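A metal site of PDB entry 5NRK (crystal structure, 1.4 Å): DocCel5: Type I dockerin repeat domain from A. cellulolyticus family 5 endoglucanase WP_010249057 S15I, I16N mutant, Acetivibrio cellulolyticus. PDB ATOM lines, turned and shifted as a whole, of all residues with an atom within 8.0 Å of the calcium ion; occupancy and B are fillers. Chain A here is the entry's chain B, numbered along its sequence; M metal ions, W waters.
The backbone NH (N) of Leu 41 lies close to the side-chain carboxylate (OD1) of Asp 51 (2.8 Å).
The side-chain carboxylate of Asp 51 sits close to the backbone NH of Asn 48, at 2.8 Å.
OD2 of Asp 40 is in hydrogen-bond range of N of Lys 45 (2.8 Å).
N of Gly 43 sits close to OD2 of Asp 40 (3.4 Å).
Water W1 lies within hydrogen-bond range of the side-chain carboxylate of Asp 44 (2.7 Å), the side-chain amide oxygen of Asn 48 (2.8 Å) and the side-chain amide nitrogen of Asn 42 (3.0 Å).
The calcium ion is bound by OD1 of Asp 40.
The calcium ion is bound by the side-chain carboxylate (OD1) of Asp 44, 2.3 Å away.
The backbone carbonyl oxygen (O) of Ser 46 binds the calcium ion (2.4 Å).
The side-chain amide oxygen (OD1) of Asn 42 binds the calcium ion.
Water W1 is bound to the calcium ion.
OD1 of Asp 51 binds the calcium ion (2.5 Å).
The calcium ion is bound by the side-chain carboxylate (OD2) of Asp 51, at 2.5 Å.
The calcium ion has seven donor atoms within binding distance.
Within 4 Å of the calcium ion: Asp 40, Asn 42, Asp 44, Ser 46 and Asp 51.
The nearest printed residue that does not touch the calcium ion is Leu 41 (4.3 Å).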
ATOM      1  N   MET A  19      -6.905 -27.783  16.293  1.00  0.00           N
ATOM      2  CA  MET A  19      -7.580 -26.508  16.526  1.00  0.00           C
ATOM      3  C   MET A  19      -8.796 -26.683  17.431  1.00  0.00           C
ATOM      4  O   MET A  19      -9.008 -25.881  18.352  1.00  0.00           O
ATOM      5  CB  MET A  19      -7.929 -25.835  15.208  1.00  0.00           C
ATOM      6  CG  MET A  19      -8.828 -24.622  15.328  1.00  0.00           C
ATOM      7  SD  MET A  19      -7.859 -23.209  15.814  1.00  0.00           S
ATOM      8  CE  MET A  19      -6.939 -22.853  14.297  1.00  0.00           C
ATOM      9  N   ILE A  36       0.679 -18.173  16.252  1.00  0.00           N
ATOM     10  CA  ILE A  36      -0.188 -17.196  15.629  1.00  0.00           C
ATOM     11  C   ILE A  36      -0.071 -17.311  14.112  1.00  0.00           C
ATOM     12  O   ILE A  36      -1.065 -17.326  13.416  1.00  0.00           O
ATOM     13  CB  ILE A  36       0.109 -15.751  16.101  1.00  0.00           C
ATOM     14  CG1 ILE A  36      -0.114 -15.608  17.609  1.00  0.00           C
ATOM     15  CG2 ILE A  36      -0.745 -14.741  15.328  1.00  0.00           C
ATOM     16  CD1 ILE A  36      -1.517 -15.790  18.105  1.00  0.00           C
ATOM     17  N   GLY A  39      -2.000 -20.533  13.208  1.00  0.00           N
ATOM     18  CA  GLY A  39      -3.405 -20.636  13.625  1.00  0.00           C
ATOM     19  C   GLY A  39      -4.307 -19.488  13.251  1.00  0.00           C
ATOM     20  O   GLY A  39      -5.532 -19.619  13.328  1.00  0.00           O
ATOM     21  N   ASP A  40      -3.725 -18.331  12.941  1.00  0.00           N
ATOM     22  CA  ASP A  40      -4.498 -17.124  12.625  1.00  0.00           C
ATOM     23  C   ASP A  40      -4.709 -17.056  11.120  1.00  0.00           C
ATOM     24  O   ASP A  40      -3.811 -16.662  10.362  1.00  0.00           O
ATOM     25  CB  ASP A  40      -3.810 -15.871  13.131  1.00  0.00           C
ATOM     26  CG  ASP A  40      -4.561 -14.635  12.817  1.00  0.00           C
ATOM     27  OD1 ASP A  40      -5.806 -14.690  12.691  1.00  0.00           O
ATOM     28  OD2 ASP A  40      -3.898 -13.567  12.697  1.00  0.00           O
ATOM     29  N   LEU A  41      -5.906 -17.404  10.708  1.00  0.00           N
ATOM     30  CA  LEU A  41      -6.215 -17.568   9.294  1.00  0.00           C
ATOM     31  C   LEU A  41      -6.939 -16.379   8.699  1.00  0.00           C
ATOM     32  O   LEU A  41      -7.156 -16.330   7.483  1.00  0.00           O
ATOM     33  CB  LEU A  41      -7.021 -18.825   9.069  1.00  0.00           C
ATOM     34  CG  LEU A  41      -6.400 -20.098   9.637  1.00  0.00           C
ATOM     35  CD1 LEU A  41      -7.258 -21.311   9.327  1.00  0.00           C
ATOM     36  CD2 LEU A  41      -4.976 -20.324   9.100  1.00  0.00           C
ATOM     37  N   ASN A  42      -7.280 -15.402   9.526  1.00  0.00           N
ATOM     38  CA  ASN A  42      -7.879 -14.134   9.052  1.00  0.00           C
ATOM     39  C   ASN A  42      -7.089 -12.885   9.392  1.00  0.00           C
ATOM     40  O   ASN A  42      -7.527 -11.789   9.061  1.00  0.00           O
ATOM     41  CB  ASN A  42      -9.338 -14.019   9.509  1.00  0.00           C
ATOM     42  CG  ASN A  42      -9.494 -14.128  10.995  1.00  0.00           C
ATOM     43  OD1 ASN A  42      -8.514 -14.096  11.718  1.00  0.00           O
ATOM     44  ND2 ASN A  42     -10.734 -14.252  11.470  1.00  0.00           N
ATOM     45  N   GLY A  43      -5.914 -13.017  10.018  1.00  0.00           N
ATOM     46  CA  GLY A  43      -5.031 -11.881  10.213  1.00  0.00           C
ATOM     47  C   GLY A  43      -5.368 -10.943  11.352  1.00  0.00           C
ATOM     48  O   GLY A  43      -4.801  -9.845  11.434  1.00  0.00           O
ATOM     49  N   ASP A  44      -6.274 -11.355  12.243  1.00  0.00           N
ATOM     50  CA  ASP A  44      -6.609 -10.507  13.393  1.00  0.00           C
ATOM     51  C   ASP A  44      -5.680 -10.713  14.611  1.00  0.00           C
ATOM     52  O   ASP A  44      -5.886 -10.097  15.650  1.00  0.00           O
ATOM     53  CB  ASP A  44      -8.097 -10.610  13.773  1.00  0.00           C
ATOM     54  CG  ASP A  44      -8.499 -11.973  14.314  1.00  0.00           C
ATOM     55  OD1 ASP A  44      -7.639 -12.870  14.423  1.00  0.00           O
ATOM     56  OD2 ASP A  44      -9.700 -12.138  14.618  1.00  0.00           O
ATOM     57  N   LYS A  45      -4.675 -11.571  14.449  1.00  0.00           N
ATOM     58  CA  LYS A  45      -3.662 -11.862  15.476  1.00  0.00           C
ATOM     59  C   LYS A  45      -4.213 -12.625  16.689  1.00  0.00           C
ATOM     60  O   LYS A  45      -3.564 -12.699  17.731  1.00  0.00           O
ATOM     61  CB  LYS A  45      -2.889 -10.596  15.896  1.00  0.00           C
ATOM     62  CG  LYS A  45      -2.276  -9.813  14.752  1.00  0.00           C
ATOM     63  CD  LYS A  45      -1.009 -10.483  14.296  1.00  0.00           C
ATOM     64  CE  LYS A  45      -0.296  -9.684  13.224  1.00  0.00           C
ATOM     65  NZ  LYS A  45      -1.073  -9.565  11.958  1.00  0.00           N
ATOM     66  N   SER A  46      -5.383 -13.219  16.535  1.00  0.00           N
ATOM     67  CA  SER A  46      -6.024 -14.062  17.548  1.00  0.00           C
ATOM     68  C   SER A  46      -6.305 -15.415  16.923  1.00  0.00           C
ATOM     69  O   SER A  46      -6.545 -15.508  15.719  1.00  0.00           O
ATOM     70  CB  SER A  46      -7.371 -13.478  18.036  1.00  0.00           C
ATOM     71  OG  SER A  46      -7.251 -12.262  18.761  1.00  0.00           O
ATOM     72  N   ILE A  47      -6.307 -16.469  17.735  1.00  0.00           N
ATOM     73  CA  ILE A  47      -6.728 -17.785  17.296  1.00  0.00           C
ATOM     74  C   ILE A  47      -8.036 -18.090  17.982  1.00  0.00           C
ATOM     75  O   ILE A  47      -8.072 -18.257  19.221  1.00  0.00           O
ATOM     76  CB  ILE A  47      -5.711 -18.889  17.657  1.00  0.00           C
ATOM     77  CG1 ILE A  47      -4.322 -18.563  17.070  1.00  0.00           C
ATOM     78  CG2 ILE A  47      -6.194 -20.225  17.149  1.00  0.00           C
ATOM     79  CD1 ILE A  47      -3.242 -19.501  17.567  1.00  0.00           C
ATOM     80  N   ASN A  48      -9.115 -18.154  17.215  1.00  0.00           N
ATOM     81  CA  ASN A  48     -10.433 -18.378  17.827  1.00  0.00           C
ATOM     82  C   ASN A  48     -11.357 -19.089  16.862  1.00  0.00           C
ATOM     83  O   ASN A  48     -10.907 -19.631  15.844  1.00  0.00           O
ATOM     84  CB  ASN A  48     -10.999 -17.058  18.365  1.00  0.00           C
ATOM     85  CG  ASN A  48     -11.231 -16.025  17.290  1.00  0.00           C
ATOM     86  OD1 ASN A  48     -11.537 -16.352  16.152  1.00  0.00           O
ATOM     87  ND2 ASN A  48     -11.102 -14.743  17.670  1.00  0.00           N
ATOM     88  N   SER A  49     -12.641 -19.138  17.173  1.00  0.00           N
ATOM     89  CA  SER A  49     -13.565 -19.925  16.380  1.00  0.00           C
ATOM     90  C   SER A  49     -13.750 -19.443  14.950  1.00  0.00           C
ATOM     91  O   SER A  49     -14.150 -20.215  14.089  1.00  0.00           O
ATOM     92  CB  SER A  49     -14.916 -20.097  17.089  1.00  0.00           C
ATOM     93  OG  SER A  49     -15.541 -18.854  17.319  1.00  0.00           O
ATOM     94  N   LEU A  50     -13.420 -18.188  14.655  1.00  0.00           N
ATOM     95  CA  LEU A  50     -13.410 -17.721  13.270  1.00  0.00           C
ATOM     96  C   LEU A  50     -12.346 -18.456  12.466  1.00  0.00           C
ATOM     97  O   LEU A  50     -12.564 -18.857  11.310  1.00  0.00           O
ATOM     98  CB  LEU A  50     -13.142 -16.209  13.179  1.00  0.00           C
ATOM     99  CG  LEU A  50     -14.110 -15.254  13.856  1.00  0.00           C
ATOM    100  CD1 LEU A  50     -13.715 -13.807  13.612  1.00  0.00           C
ATOM    101  CD2 LEU A  50     -15.488 -15.484  13.333  1.00  0.00           C
ATOM    102  N   ASP A  51     -11.188 -18.641  13.072  1.00  0.00           N
ATOM    103  CA  ASP A  51     -10.109 -19.403  12.420  1.00  0.00           C
ATOM    104  C   ASP A  51     -10.505 -20.865  12.206  1.00  0.00           C
ATOM    105  O   ASP A  51     -10.224 -21.453  11.156  1.00  0.00           O
ATOM    106  CB  ASP A  51      -8.833 -19.286  13.222  1.00  0.00           C
ATOM    107  CG  ASP A  51      -8.469 -17.844  13.433  1.00  0.00           C
ATOM    108  OD1 ASP A  51      -8.080 -17.165  12.448  1.00  0.00           O
ATOM    109  OD2 ASP A  51      -8.581 -17.338  14.558  1.00  0.00           O
ATOM    110  N   PHE A  52     -11.182 -21.448  13.193  1.00  0.00           N
ATOM    111  CA  PHE A  52     -11.688 -22.812  13.105  1.00  0.00           C
ATOM    112  C   PHE A  52     -12.648 -22.963  11.911  1.00  0.00           C
ATOM    113  O   PHE A  52     -12.570 -23.922  11.144  1.00  0.00           O
ATOM    114  CB  PHE A  52     -12.325 -23.134  14.454  1.00  0.00           C
ATOM    115  CG  PHE A  52     -12.773 -24.555  14.660  1.00  0.00           C
ATOM    116  CD1 PHE A  52     -11.928 -25.641  14.451  1.00  0.00           C
ATOM    117  CD2 PHE A  52     -14.039 -24.805  15.154  1.00  0.00           C
ATOM    118  CE1 PHE A  52     -12.360 -26.921  14.731  1.00  0.00           C
ATOM    119  CE2 PHE A  52     -14.468 -26.092  15.422  1.00  0.00           C
ATOM    120  CZ  PHE A  52     -13.640 -27.148  15.172  1.00  0.00           C
ATOM    121  N   ILE A  54     -12.723 -21.024   9.241  1.00  0.00           N
ATOM    122  CA  ILE A  54     -11.986 -20.853   8.007  1.00  0.00           C
ATOM    123  C   ILE A  54     -11.269 -22.164   7.626  1.00  0.00           C
ATOM    124  O   ILE A  54     -11.266 -22.579   6.459  1.00  0.00           O
ATOM    125  CB  ILE A  54     -11.001 -19.680   8.112  1.00  0.00           C
ATOM    126  CG1 ILE A  54     -11.774 -18.366   8.210  1.00  0.00           C
ATOM    127  CG2 ILE A  54     -10.040 -19.667   6.922  1.00  0.00           C
ATOM    128  CD1 ILE A  54     -10.945 -17.197   8.708  1.00  0.00           C
ATOM    129  N   VAL A  68      -4.539 -14.237   4.455  1.00  0.00           N
ATOM    130  CA  VAL A  68      -3.604 -14.328   5.590  1.00  0.00           C
ATOM    131  C   VAL A  68      -3.898 -13.469   6.818  1.00  0.00           C
ATOM    132  O   VAL A  68      -3.610 -13.903   7.945  1.00  0.00           O
ATOM    133  CB  VAL A  68      -2.134 -14.154   5.088  1.00  0.00           C
ATOM    134  CG1 VAL A  68      -1.195 -13.631   6.166  1.00  0.00           C
ATOM    135  CG2 VAL A  68      -1.605 -15.460   4.524  1.00  0.00           C
HETATM  136 CA    CA M   1      -7.796 -15.114  13.766  1.00  0.00          CA
HETATM  137  O   HOH W   1     -10.106 -14.768  14.390  1.00  0.00           O
